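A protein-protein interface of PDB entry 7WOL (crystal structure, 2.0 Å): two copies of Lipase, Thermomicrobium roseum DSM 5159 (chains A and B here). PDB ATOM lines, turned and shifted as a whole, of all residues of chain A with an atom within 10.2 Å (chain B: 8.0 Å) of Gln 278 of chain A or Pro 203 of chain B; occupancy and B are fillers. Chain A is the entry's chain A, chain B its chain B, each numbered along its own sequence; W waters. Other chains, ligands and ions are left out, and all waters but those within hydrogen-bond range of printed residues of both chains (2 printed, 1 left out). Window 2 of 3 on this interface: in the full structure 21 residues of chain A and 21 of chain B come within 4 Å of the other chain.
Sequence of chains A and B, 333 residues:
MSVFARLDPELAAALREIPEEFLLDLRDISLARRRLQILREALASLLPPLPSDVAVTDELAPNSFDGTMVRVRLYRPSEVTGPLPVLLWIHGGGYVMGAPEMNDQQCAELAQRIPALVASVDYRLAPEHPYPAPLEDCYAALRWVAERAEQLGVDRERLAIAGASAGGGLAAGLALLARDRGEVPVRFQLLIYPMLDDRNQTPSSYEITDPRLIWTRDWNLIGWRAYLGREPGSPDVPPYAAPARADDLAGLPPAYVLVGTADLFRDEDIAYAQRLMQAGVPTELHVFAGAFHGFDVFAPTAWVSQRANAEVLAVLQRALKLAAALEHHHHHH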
ATOM      1  N   ALA A 246      29.942 -18.341 -18.055  1.00  0.00           N
ATOM      2  CA  ALA A 246      30.655 -17.777 -16.893  1.00  0.00           C
ATOM      3  C   ALA A 246      29.857 -18.113 -15.636  1.00  0.00           C
ATOM      4  O   ALA A 246      28.640 -17.862 -15.620  1.00  0.00           O
ATOM      5  CB  ALA A 246      30.833 -16.292 -17.035  1.00  0.00           C
ATOM      6  N   ASP A 247      30.525 -18.648 -14.620  1.00  0.00           N
ATOM      7  CA  ASP A 247      29.896 -19.078 -13.345  1.00  0.00           C
ATOM      8  C   ASP A 247      29.644 -17.841 -12.477  1.00  0.00           C
ATOM      9  O   ASP A 247      28.503 -17.631 -12.078  1.00  0.00           O
ATOM     10  CB  ASP A 247      30.768 -20.129 -12.649  1.00  0.00           C
ATOM     11  CG  ASP A 247      30.252 -20.556 -11.284  1.00  0.00           C
ATOM     12  OD1 ASP A 247      29.043 -20.357 -11.020  1.00  0.00           O
ATOM     13  OD2 ASP A 247      31.065 -21.094 -10.490  1.00  0.00           O
ATOM     14  N   ASP A 248      30.671 -17.038 -12.215  1.00  0.00           N
ATOM     15  CA  ASP A 248      30.612 -15.937 -11.220  1.00  0.00           C
ATOM     16  C   ASP A 248      30.579 -14.593 -11.959  1.00  0.00           C
ATOM     17  O   ASP A 248      31.595 -14.214 -12.565  1.00  0.00           O
ATOM     18  CB  ASP A 248      31.773 -15.988 -10.229  1.00  0.00           C
ATOM     19  CG  ASP A 248      31.807 -14.757  -9.346  1.00  0.00           C
ATOM     20  OD1 ASP A 248      30.719 -14.359  -8.849  1.00  0.00           O
ATOM     21  OD2 ASP A 248      32.903 -14.169  -9.222  1.00  0.00           O
ATOM     22  N   LEU A 249      29.435 -13.907 -11.892  1.00  0.00           N
ATOM     23  CA  LEU A 249      29.178 -12.643 -12.611  1.00  0.00           C
ATOM     24  C   LEU A 249      29.300 -11.459 -11.650  1.00  0.00           C
ATOM     25  O   LEU A 249      29.106 -10.319 -12.119  1.00  0.00           O
ATOM     26  CB  LEU A 249      27.789 -12.713 -13.245  1.00  0.00           C
ATOM     27  CG  LEU A 249      27.547 -13.798 -14.295  1.00  0.00           C
ATOM     28  CD1 LEU A 249      26.180 -13.613 -14.950  1.00  0.00           C
ATOM     29  CD2 LEU A 249      28.613 -13.814 -15.387  1.00  0.00           C
ATOM     30  N   ALA A 250      29.611 -11.681 -10.361  1.00  0.00           N
ATOM     31  CA  ALA A 250      29.675 -10.598  -9.358  1.00  0.00           C
ATOM     32  C   ALA A 250      30.771  -9.588  -9.751  1.00  0.00           C
ATOM     33  O   ALA A 250      31.798 -10.008 -10.300  1.00  0.00           O
ATOM     34  CB  ALA A 250      29.904 -11.154  -7.961  1.00  0.00           C
ATOM     35  N   GLY A 251      30.544  -8.302  -9.485  1.00  0.00           N
ATOM     36  CA  GLY A 251      31.540  -7.240  -9.700  1.00  0.00           C
ATOM     37  C   GLY A 251      31.649  -6.837 -11.171  1.00  0.00           C
ATOM     38  O   GLY A 251      32.573  -6.092 -11.494  1.00  0.00           O
ATOM     39  N   ILE A 270      18.044 -13.359 -21.902  1.00  0.00           N
ATOM     40  CA  ILE A 270      17.228 -13.235 -20.666  1.00  0.00           C
ATOM     41  C   ILE A 270      18.008 -13.916 -19.533  1.00  0.00           C
ATOM     42  O   ILE A 270      18.124 -13.325 -18.476  1.00  0.00           O
ATOM     43  CB  ILE A 270      15.829 -13.843 -20.857  1.00  0.00           C
ATOM     44  CG1 ILE A 270      14.967 -12.994 -21.806  1.00  0.00           C
ATOM     45  CG2 ILE A 270      15.173 -14.036 -19.511  1.00  0.00           C
ATOM     46  CD1 ILE A 270      13.695 -13.685 -22.313  1.00  0.00           C
ATOM     47  N   ALA A 271      18.558 -15.101 -19.778  1.00  0.00           N
ATOM     48  CA  ALA A 271      19.243 -15.897 -18.734  1.00  0.00           C
ATOM     49  C   ALA A 271      20.494 -15.144 -18.268  1.00  0.00           C
ATOM     50  O   ALA A 271      20.717 -15.041 -17.051  1.00  0.00           O
ATOM     51  CB  ALA A 271      19.554 -17.280 -19.260  1.00  0.00           C
ATOM     52  N   TYR A 272      21.261 -14.551 -19.189  1.00  0.00           N
ATOM     53  CA  TYR A 272      22.487 -13.798 -18.815  1.00  0.00           C
ATOM     54  C   TYR A 272      22.083 -12.594 -17.963  1.00  0.00           C
ATOM     55  O   TYR A 272      22.680 -12.371 -16.886  1.00  0.00           O
ATOM     56  CB  TYR A 272      23.290 -13.351 -20.041  1.00  0.00           C
ATOM     57  CG  TYR A 272      24.690 -12.909 -19.701  1.00  0.00           C
ATOM     58  CD1 TYR A 272      25.646 -13.838 -19.315  1.00  0.00           C
ATOM     59  CD2 TYR A 272      25.059 -11.570 -19.726  1.00  0.00           C
ATOM     60  CE1 TYR A 272      26.940 -13.445 -18.986  1.00  0.00           C
ATOM     61  CE2 TYR A 272      26.352 -11.161 -19.399  1.00  0.00           C
ATOM     62  CZ  TYR A 272      27.297 -12.100 -19.021  1.00  0.00           C
ATOM     63  OH  TYR A 272      28.572 -11.714 -18.699  1.00  0.00           O
ATOM     64  N   ALA A 273      21.066 -11.842 -18.397  1.00  0.00           N
ATOM     65  CA  ALA A 273      20.568 -10.651 -17.662  1.00  0.00           C
ATOM     66  C   ALA A 273      20.102 -11.056 -16.252  1.00  0.00           C
ATOM     67  O   ALA A 273      20.425 -10.373 -15.270  1.00  0.00           O
ATOM     68  CB  ALA A 273      19.454  -9.970 -18.431  1.00  0.00           C
ATOM     69  N   GLN A 274      19.327 -12.125 -16.146  1.00  0.00           N
ATOM     70  CA  GLN A 274      18.798 -12.570 -14.834  1.00  0.00           C
ATOM     71  C   GLN A 274      19.952 -13.031 -13.928  1.00  0.00           C
ATOM     72  O   GLN A 274      19.877 -12.763 -12.725  1.00  0.00           O
ATOM     73  CB  GLN A 274      17.801 -13.704 -15.035  1.00  0.00           C
ATOM     74  CG  GLN A 274      17.107 -14.090 -13.742  1.00  0.00           C
ATOM     75  CD  GLN A 274      15.942 -15.023 -13.962  1.00  0.00           C
ATOM     76  OE1 GLN A 274      15.838 -15.705 -14.985  1.00  0.00           O
ATOM     77  NE2 GLN A 274      15.046 -15.032 -12.992  1.00  0.00           N
ATOM     78  N   ARG A 275      20.946 -13.742 -14.464  1.00  0.00           N
ATOM     79  CA  ARG A 275      22.132 -14.191 -13.681  1.00  0.00           C
ATOM     80  C   ARG A 275      22.951 -12.968 -13.230  1.00  0.00           C
ATOM     81  O   ARG A 275      23.402 -12.960 -12.069  1.00  0.00           O
ATOM     82  CB  ARG A 275      22.928 -15.236 -14.467  1.00  0.00           C
ATOM     83  CG  ARG A 275      22.198 -16.572 -14.585  1.00  0.00           C
ATOM     84  CD  ARG A 275      23.145 -17.754 -14.532  1.00  0.00           C
ATOM     85  NE  ARG A 275      24.094 -17.582 -15.590  1.00  0.00           N
ATOM     86  CZ  ARG A 275      25.407 -17.487 -15.466  1.00  0.00           C
ATOM     87  NH1 ARG A 275      26.130 -17.294 -16.558  1.00  0.00           N
ATOM     88  NH2 ARG A 275      25.997 -17.626 -14.294  1.00  0.00           N
ATOM     89  N   LEU A 276      23.106 -11.927 -14.063  1.00  0.00           N
ATOM     90  CA  LEU A 276      23.696 -10.647 -13.589  1.00  0.00           C
ATOM     91  C   LEU A 276      22.923 -10.148 -12.372  1.00  0.00           C
ATOM     92  O   LEU A 276      23.581  -9.804 -11.351  1.00  0.00           O
ATOM     93  CB  LEU A 276      23.695  -9.595 -14.696  1.00  0.00           C
ATOM     94  CG  LEU A 276      24.678  -9.841 -15.831  1.00  0.00           C
ATOM     95  CD1 LEU A 276      24.335  -8.938 -17.014  1.00  0.00           C
ATOM     96  CD2 LEU A 276      26.112  -9.609 -15.358  1.00  0.00           C
ATOM     97  N   MET A 277      21.589 -10.065 -12.465  1.00  0.00           N
ATOM     98  CA  MET A 277      20.754  -9.513 -11.369  1.00  0.00           C
ATOM     99  C   MET A 277      20.968 -10.378 -10.121  1.00  0.00           C
ATOM    100  O   MET A 277      21.077  -9.832  -9.025  1.00  0.00           O
ATOM    101  CB  MET A 277      19.263  -9.513 -11.720  1.00  0.00           C
ATOM    102  CG  MET A 277      18.910  -8.603 -12.877  1.00  0.00           C
ATOM    103  SD  MET A 277      17.300  -9.097 -13.553  1.00  0.00           S
ATOM    104  CE  MET A 277      17.324  -8.211 -15.116  1.00  0.00           C
ATOM    105  N   GLN A 278      21.044 -11.685 -10.298  1.00  0.00           N
ATOM    106  CA  GLN A 278      21.181 -12.614  -9.144  1.00  0.00           C
ATOM    107  C   GLN A 278      22.580 -12.465  -8.535  1.00  0.00           C
ATOM    108  O   GLN A 278      22.707 -12.774  -7.356  1.00  0.00           O
ATOM    109  CB  GLN A 278      20.856 -14.037  -9.573  1.00  0.00           C
ATOM    110  CG  GLN A 278      19.361 -14.224  -9.763  1.00  0.00           C
ATOM    111  CD  GLN A 278      18.995 -15.561 -10.347  1.00  0.00           C
ATOM    112  OE1 GLN A 278      19.847 -16.329 -10.788  1.00  0.00           O
ATOM    113  NE2 GLN A 278      17.698 -15.817 -10.407  1.00  0.00           N
ATOM    114  N   ALA A 279      23.569 -11.950  -9.273  1.00  0.00           N
ATOM    115  CA  ALA A 279      24.951 -11.758  -8.770  1.00  0.00           C
ATOM    116  C   ALA A 279      25.094 -10.355  -8.179  1.00  0.00           C
ATOM    117  O   ALA A 279      26.198 -10.019  -7.796  1.00  0.00           O
ATOM    118  CB  ALA A 279      25.963 -12.029  -9.863  1.00  0.00           C
ATOM    119  N   GLY A 280      24.009  -9.578  -8.116  1.00  0.00           N
ATOM    120  CA  GLY A 280      23.984  -8.215  -7.555  1.00  0.00           C
ATOM    121  C   GLY A 280      24.495  -7.154  -8.529  1.00  0.00           C
ATOM    122  O   GLY A 280      24.722  -6.028  -8.100  1.00  0.00           O
ATOM    123  N   VAL A 281      24.616  -7.450  -9.819  1.00  0.00           N
ATOM    124  CA  VAL A 281      24.991  -6.413 -10.833  1.00  0.00           C
ATOM    125  C   VAL A 281      23.729  -5.658 -11.223  1.00  0.00           C
ATOM    126  O   VAL A 281      22.770  -6.278 -11.662  1.00  0.00           O
ATOM    127  CB  VAL A 281      25.639  -7.072 -12.055  1.00  0.00           C
ATOM    128  CG1 VAL A 281      25.962  -6.059 -13.141  1.00  0.00           C
ATOM    129  CG2 VAL A 281      26.861  -7.879 -11.648  1.00  0.00           C
ATOM    130  N   PRO A 282      23.666  -4.320 -11.065  1.00  0.00           N
ATOM    131  CA  PRO A 282      22.489  -3.561 -11.477  1.00  0.00           C
ATOM    132  C   PRO A 282      22.272  -3.744 -12.982  1.00  0.00           C
ATOM    133  O   PRO A 282      23.198  -3.493 -13.758  1.00  0.00           O
ATOM    134  CB  PRO A 282      22.842  -2.095 -11.169  1.00  0.00           C
ATOM    135  CG  PRO A 282      23.956  -2.182 -10.127  1.00  0.00           C
ATOM    136  CD  PRO A 282      24.687  -3.477 -10.422  1.00  0.00           C
ATOM    137  N   THR A 283      21.106  -4.250 -13.372  1.00  0.00           N
ATOM    138  CA  THR A 283      20.850  -4.717 -14.755  1.00  0.00           C
ATOM    139  C   THR A 283      19.432  -4.328 -15.152  1.00  0.00           C
ATOM    140  O   THR A 283      18.483  -4.630 -14.390  1.00  0.00           O
ATOM    141  CB  THR A 283      21.086  -6.230 -14.911  1.00  0.00           C
ATOM    142  OG1 THR A 283      22.425  -6.533 -14.519  1.00  0.00           O
ATOM    143  CG2 THR A 283      20.873  -6.734 -16.323  1.00  0.00           C
ATOM    144  N   GLU A 284      19.324  -3.662 -16.296  1.00  0.00           N
ATOM    145  CA  GLU A 284      18.065  -3.402 -17.008  1.00  0.00           C
ATOM    146  C   GLU A 284      17.953  -4.393 -18.172  1.00  0.00           C
ATOM    147  O   GLU A 284      18.919  -4.590 -18.938  1.00  0.00           O
ATOM    148  CB  GLU A 284      18.026  -1.927 -17.391  1.00  0.00           C
ATOM    149  CG  GLU A 284      16.767  -1.579 -18.155  1.00  0.00           C
ATOM    150  CD  GLU A 284      16.551  -0.118 -18.514  1.00  0.00           C
ATOM    151  OE1 GLU A 284      17.200   0.769 -17.905  1.00  0.00           O
ATOM    152  OE2 GLU A 284      15.680   0.121 -19.389  1.00  0.00           O
ATOM    153  N   ASN B 200       7.234 -19.138  -3.073  1.00  0.00           N
ATOM    154  CA  ASN B 200       8.313 -18.381  -2.396  1.00  0.00           C
ATOM    155  C   ASN B 200       9.606 -19.200  -2.412  1.00  0.00           C
ATOM    156  O   ASN B 200      10.255 -19.350  -1.343  1.00  0.00           O
ATOM    157  CB  ASN B 200       7.897 -17.992  -0.976  1.00  0.00           C
ATOM    158  CG  ASN B 200       6.933 -16.830  -0.979  1.00  0.00           C
ATOM    159  OD1 ASN B 200       7.352 -15.679  -0.878  1.00  0.00           O
ATOM    160  ND2 ASN B 200       5.658 -17.123  -1.178  1.00  0.00           N
ATOM    161  N   GLN B 201       9.996 -19.697  -3.580  1.00  0.00           N
ATOM    162  CA  GLN B 201      11.228 -20.511  -3.703  1.00  0.00           C
ATOM    163  C   GLN B 201      12.241 -19.846  -4.644  1.00  0.00           C
ATOM    164  O   GLN B 201      13.344 -20.363  -4.708  1.00  0.00           O
ATOM    165  CB  GLN B 201      10.884 -21.952  -4.078  1.00  0.00           C
ATOM    166  CG  GLN B 201      10.019 -22.066  -5.312  1.00  0.00           C
ATOM    167  CD  GLN B 201       9.487 -23.450  -5.593  1.00  0.00           C
ATOM    168  OE1 GLN B 201       9.055 -23.719  -6.706  1.00  0.00           O
ATOM    169  NE2 GLN B 201       9.516 -24.327  -4.599  1.00  0.00           N
ATOM    170  N   THR B 202      11.934 -18.730  -5.321  1.00  0.00           N
ATOM    171  CA  THR B 202      12.917 -18.088  -6.237  1.00  0.00           C
ATOM    172  C   THR B 202      13.992 -17.379  -5.414  1.00  0.00           C
ATOM    173  O   THR B 202      13.775 -16.996  -4.244  1.00  0.00           O
ATOM    174  CB  THR B 202      12.261 -17.073  -7.179  1.00  0.00           C
ATOM    175  OG1 THR B 202      11.708 -16.085  -6.304  1.00  0.00           O
ATOM    176  CG2 THR B 202      11.235 -17.692  -8.103  1.00  0.00           C
ATOM    177  N   PRO B 203      15.179 -17.139  -6.005  1.00  0.00           N
ATOM    178  CA  PRO B 203      16.213 -16.359  -5.325  1.00  0.00           C
ATOM    179  C   PRO B 203      15.724 -14.993  -4.828  1.00  0.00           C
ATOM    180  O   PRO B 203      15.963 -14.687  -3.660  1.00  0.00           O
ATOM    181  CB  PRO B 203      17.327 -16.255  -6.384  1.00  0.00           C
ATOM    182  CG  PRO B 203      17.166 -17.535  -7.191  1.00  0.00           C
ATOM    183  CD  PRO B 203      15.667 -17.749  -7.255  1.00  0.00           C
ATOM    184  N   SER B 204      15.021 -14.214  -5.666  1.00  0.00           N
ATOM    185  CA  SER B 204      14.518 -12.877  -5.258  1.00  0.00           C
ATOM    186  C   SER B 204      13.537 -12.986  -4.080  1.00  0.00           C
ATOM    187  O   SER B 204      13.470 -12.006  -3.269  1.00  0.00           O
ATOM    188  CB  SER B 204      13.919 -12.081  -6.404  1.00  0.00           C
ATOM    189  OG  SER B 204      12.797 -12.725  -6.990  1.00  0.00           O
ATOM    190  N   SER B 205      12.784 -14.083  -3.961  1.00  0.00           N
ATOM    191  CA  SER B 205      11.788 -14.247  -2.858  1.00  0.00           C
ATOM    192  C   SER B 205      12.483 -14.331  -1.483  1.00  0.00           C
ATOM    193  O   SER B 205      11.777 -14.151  -0.449  1.00  0.00           O
ATOM    194  CB  SER B 205      10.831 -15.413  -3.074  1.00  0.00           C
ATOM    195  OG  SER B 205      11.437 -16.665  -2.824  1.00  0.00           O
ATOM    196  N   TYR B 206      13.804 -14.513  -1.438  1.00  0.00           N
ATOM    197  CA  TYR B 206      14.585 -14.506  -0.173  1.00  0.00           C
ATOM    198  C   TYR B 206      15.304 -13.172   0.020  1.00  0.00           C
ATOM    199  O   TYR B 206      15.772 -12.935   1.129  1.00  0.00           O
ATOM    200  CB  TYR B 206      15.592 -15.657  -0.143  1.00  0.00           C
ATOM    201  CG  TYR B 206      14.946 -17.011  -0.041  1.00  0.00           C
ATOM    202  CD1 TYR B 206      14.611 -17.560   1.191  1.00  0.00           C
ATOM    203  CD2 TYR B 206      14.637 -17.735  -1.178  1.00  0.00           C
ATOM    204  CE1 TYR B 206      14.001 -18.806   1.283  1.00  0.00           C
ATOM    205  CE2 TYR B 206      14.034 -18.985  -1.103  1.00  0.00           C
ATOM    206  CZ  TYR B 206      13.710 -19.521   0.133  1.00  0.00           C
ATOM    207  OH  TYR B 206      13.118 -20.752   0.194  1.00  0.00           O
ATOM    208  N   GLU B 207      15.363 -12.311  -0.997  1.00  0.00           N
ATOM    209  CA  GLU B 207      16.309 -11.169  -1.021  1.00  0.00           C
ATOM    210  C   GLU B 207      15.735  -9.978  -0.244  1.00  0.00           C
ATOM    211  O   GLU B 207      16.540  -9.158   0.203  1.00  0.00           O
ATOM    212  CB  GLU B 207      16.672 -10.784  -2.460  1.00  0.00           C
ATOM    213  CG  GLU B 207      17.636 -11.755  -3.134  1.00  0.00           C
ATOM    214  CD  GLU B 207      17.896 -11.476  -4.615  1.00  0.00           C
ATOM    215  OE1 GLU B 207      17.550 -10.374  -5.069  1.00  0.00           O
ATOM    216  OE2 GLU B 207      18.435 -12.360  -5.325  1.00  0.00           O
ATOM    217  N   ILE B 208      14.412  -9.835  -0.116  1.00  0.00           N
ATOM    218  CA  ILE B 208      13.795  -8.621   0.490  1.00  0.00           C
ATOM    219  C   ILE B 208      13.173  -9.007   1.837  1.00  0.00           C
ATOM    220  O   ILE B 208      12.108  -9.639   1.835  1.00  0.00           O
ATOM    221  CB  ILE B 208      12.761  -7.958  -0.442  1.00  0.00           C
ATOM    222  CG1 ILE B 208      13.267  -7.758  -1.876  1.00  0.00           C
ATOM    223  CG2 ILE B 208      12.300  -6.641   0.160  1.00  0.00           C
ATOM    224  CD1 ILE B 208      14.438  -6.786  -1.993  1.00  0.00           C
ATOM    225  N   ARG B 217       9.474 -10.845   2.196  1.00  0.00           N
ATOM    226  CA  ARG B 217       9.134 -12.285   2.208  1.00  0.00           C
ATOM    227  C   ARG B 217       8.065 -12.556   3.285  1.00  0.00           C
ATOM    228  O   ARG B 217       7.093 -13.261   2.981  1.00  0.00           O
ATOM    229  CB  ARG B 217      10.383 -13.120   2.456  1.00  0.00           C
ATOM    230  CG  ARG B 217      10.124 -14.618   2.413  1.00  0.00           C
ATOM    231  CD  ARG B 217      11.355 -15.470   2.645  1.00  0.00           C
ATOM    232  NE  ARG B 217      10.994 -16.890   2.513  1.00  0.00           N
ATOM    233  CZ  ARG B 217      10.902 -17.576   1.380  1.00  0.00           C
ATOM    234  NH1 ARG B 217      11.166 -17.011   0.205  1.00  0.00           N
ATOM    235  NH2 ARG B 217      10.543 -18.850   1.422  1.00  0.00           N
ATOM    236  N   THR B 261      14.616  -4.873 -10.257  1.00  0.00           N
ATOM    237  CA  THR B 261      15.608  -5.868  -9.813  1.00  0.00           C
ATOM    238  C   THR B 261      15.571  -6.029  -8.288  1.00  0.00           C
ATOM    239  O   THR B 261      15.984  -7.107  -7.840  1.00  0.00           O
ATOM    240  CB  THR B 261      17.018  -5.521 -10.284  1.00  0.00           C
ATOM    241  OG1 THR B 261      17.346  -4.271  -9.683  1.00  0.00           O
ATOM    242  CG2 THR B 261      17.121  -5.502 -11.793  1.00  0.00           C
ATOM    243  N   ASP B 263      12.969  -6.206  -6.317  1.00  0.00           N
ATOM    244  CA  ASP B 263      11.578  -6.626  -6.032  1.00  0.00           C
ATOM    245  C   ASP B 263      11.638  -8.112  -5.687  1.00  0.00           C
ATOM    246  O   ASP B 263      12.285  -8.886  -6.418  1.00  0.00           O
ATOM    247  CB  ASP B 263      10.676  -6.282  -7.215  1.00  0.00           C
ATOM    248  CG  ASP B 263       9.183  -6.355  -6.917  1.00  0.00           C
ATOM    249  OD1 ASP B 263       8.753  -7.379  -6.322  1.00  0.00           O
ATOM    250  OD2 ASP B 263       8.455  -5.408  -7.314  1.00  0.00           O
ATOM    251  N   LEU B 264      10.936  -8.501  -4.629  1.00  0.00           N
ATOM    252  CA  LEU B 264      10.708  -9.914  -4.247  1.00  0.00           C
ATOM    253  C   LEU B 264      10.274 -10.724  -5.469  1.00  0.00           C
ATOM    254  O   LEU B 264      10.634 -11.915  -5.583  1.00  0.00           O
ATOM    255  CB  LEU B 264       9.615  -9.896  -3.174  1.00  0.00           C
ATOM    256  CG  LEU B 264       9.612 -11.037  -2.177  1.00  0.00           C
ATOM    257  CD1 LEU B 264      10.820 -10.980  -1.240  1.00  0.00           C
ATOM    258  CD2 LEU B 264       8.308 -11.008  -1.385  1.00  0.00           C
ATOM    259  N   ARG B 266      10.937 -10.224  -8.697  1.00  0.00           N
ATOM    260  CA  ARG B 266      11.828 -10.146  -9.887  1.00  0.00           C
ATOM    261  C   ARG B 266      11.839 -11.492 -10.601  1.00  0.00           C
ATOM    262  O   ARG B 266      11.510 -11.538 -11.806  1.00  0.00           O
ATOM    263  CB  ARG B 266      13.241  -9.738  -9.476  1.00  0.00           C
ATOM    264  CG  ARG B 266      14.235  -9.726 -10.626  1.00  0.00           C
ATOM    265  CD  ARG B 266      15.651  -9.582 -10.110  1.00  0.00           C
ATOM    266  NE  ARG B 266      16.136 -10.829  -9.537  1.00  0.00           N
ATOM    267  CZ  ARG B 266      16.863 -10.921  -8.425  1.00  0.00           C
ATOM    268  NH1 ARG B 266      17.204  -9.834  -7.762  1.00  0.00           N
ATOM    269  NH2 ARG B 266      17.242 -12.102  -7.970  1.00  0.00           N
ATOM    270  N   ASP B 267      12.196 -12.568  -9.890  1.00  0.00           N
ATOM    271  CA  ASP B 267      12.474 -13.868 -10.548  1.00  0.00           C
ATOM    272  C   ASP B 267      11.176 -14.537 -11.028  1.00  0.00           C
ATOM    273  O   ASP B 267      11.174 -15.108 -12.144  1.00  0.00           O
ATOM    274  CB  ASP B 267      13.389 -14.731  -9.678  1.00  0.00           C
ATOM    275  CG  ASP B 267      14.803 -14.155  -9.563  1.00  0.00           C
ATOM    276  OD1 ASP B 267      15.265 -13.476 -10.519  1.00  0.00           O
ATOM    277  OD2 ASP B 267      15.414 -14.332  -8.496  1.00  0.00           O
ATOM    278  N   GLU B 268      10.088 -14.491 -10.265  1.00  0.00           N
ATOM    279  CA  GLU B 268       8.826 -15.125 -10.734  1.00  0.00           C
ATOM    280  C   GLU B 268       8.307 -14.352 -11.950  1.00  0.00           C
ATOM    281  O   GLU B 268       7.714 -14.979 -12.818  1.00  0.00           O
ATOM    282  CB  GLU B 268       7.790 -15.243  -9.617  1.00  0.00           C
ATOM    283  CG  GLU B 268       7.249 -13.950  -9.063  1.00  0.00           C
ATOM    284  CD  GLU B 268       6.661 -14.109  -7.671  1.00  0.00           C
ATOM    285  OE1 GLU B 268       7.452 -14.398  -6.747  1.00  0.00           O
ATOM    286  OE2 GLU B 268       5.424 -13.945  -7.521  1.00  0.00           O
ATOM    287  N   ILE B 270      10.039 -12.526 -14.197  1.00  0.00           N
ATOM    288  CA  ILE B 270      10.893 -12.860 -15.367  1.00  0.00           C
ATOM    289  C   ILE B 270      10.499 -14.242 -15.886  1.00  0.00           C
ATOM    290  O   ILE B 270      10.391 -14.389 -17.108  1.00  0.00           O
ATOM    291  CB  ILE B 270      12.404 -12.777 -15.060  1.00  0.00           C
ATOM    292  CG1 ILE B 270      12.877 -11.346 -14.836  1.00  0.00           C
ATOM    293  CG2 ILE B 270      13.193 -13.450 -16.174  1.00  0.00           C
ATOM    294  CD1 ILE B 270      14.257 -11.261 -14.221  1.00  0.00           C
HETATM  295  O   HOH W   1      20.222  -5.878 -10.716  1.00  0.00           O
HETATM  296  O   HOH W   2      20.639 -14.288  -6.002  1.00  0.00           O
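NE2 of Gln 274 of chain A is in hydrogen-bond range of OD1 of Asp 267 of chain B. The side-chain amide nitrogen of Gln 278 of chain A sits at hydrogen-bond distance from the side-chain carboxylate of Asp 267 of chain B (3.3 Å).
The backbone carbonyl oxygen of Val 281 of chain A is in hydrogen-bond range of the side-chain hydroxyl of Thr 283 of chain A (2.9 Å). OD2 of Asp 267 of chain B lies within hydrogen-bond range of N of Ser 204 of chain B, at 2.9 Å. The side-chain carboxylate (OE1) of Glu 207 of chain B is in salt-bridge range of the guanidinium group (NH1) of Arg 266 of chain B, at 2.8 Å. O of Thr 261 of chain B lies within hydrogen-bond range of NH1 of Arg 266 of chain B, at 3.0 Å. The side-chain carboxylate (OD2) of Asp 267 of chain B is in salt-bridge range of the guanidinium group (NH2) of Arg 266 of chain B, at 2.9 Å.
Ile 270 of chain B touches Ile 270 of chain A. Ile 270 of chain B touches Gln 274 of chain A (CG2 to OE1, 3.7 Å). Thr 261 of chain B touches Met 277 of chain A (CG2 to CG, 3.7 Å). Arg 266 of chain B touches Met 277 of chain A (CD to SD, 3.8 Å). Met 277 of chain A touches Ile 270 of chain B. CG of Pro 203 of chain B touches NE2 of Gln 278 of chain A, 3.7 Å away. Gln 278 of chain A touches Arg 266 of chain B. Thr 283 of chain A touches Thr 261 of chain B.
Of the printed residues of chain B, Ile 270 of chain A touches Ile 270 (3.9 Å). Of the printed residues of chain B, Gln 274 of chain A touches Asp 267 and Ile 270. Of the printed residues of chain B, Met 277 of chain A touches Thr 261 (3.7 Å), Arg 266 (3.8 Å) and Ile 270 (3.8 Å). Of chain B, only Pro 203 (3.7 Å), Arg 266 (3.5 Å) and Asp 267 (3.3 Å) come within 4 Å of Gln 278 of chain A. No residue of chain A comes within 4 Å of Ser 204 of chain B. Of the printed residues of chain A, Thr 261 of chain B touches Met 277 (3.7 Å) and Thr 283 (3.1 Å). Of the printed residues of chain A, Asp 267 of chain B touches Gln 274 (2.9 Å) and Gln 278 (3.3 Å). The nearest printed residue of chain A that does not touch Arg 266 of chain B is Gln 274 of chain A (5.1 Å).
Printed residues of chain B that touch a printed residue of chain A: Pro 203, Thr 261, Arg 266, Asp 267 and Ile 270. Hydrophobic or aromatic side chains of chain B that line the printed part of chain A: Pro 203 and Ile 270. Along chain B the printed residues that touch a printed residue of chain A span positions 203 to 270. Among the printed residues, 10 pairs touch across the chains.
Ile 270 of chain A touches its own counterpart, Ile 270 of chain B.
Water W1 lies within hydrogen-bond range of the backbone carbonyl oxygen (O) of Val 281 of chain A, the backbone NH (N) of Thr 283 of chain A and the side-chain hydroxyl (OG1) of Thr 261 of chain B. Water W2 lies within hydrogen-bond range of O of Gln 278 of chain A (2.9 Å) and OE2 of Glu 207 of chain B (3.0 Å).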
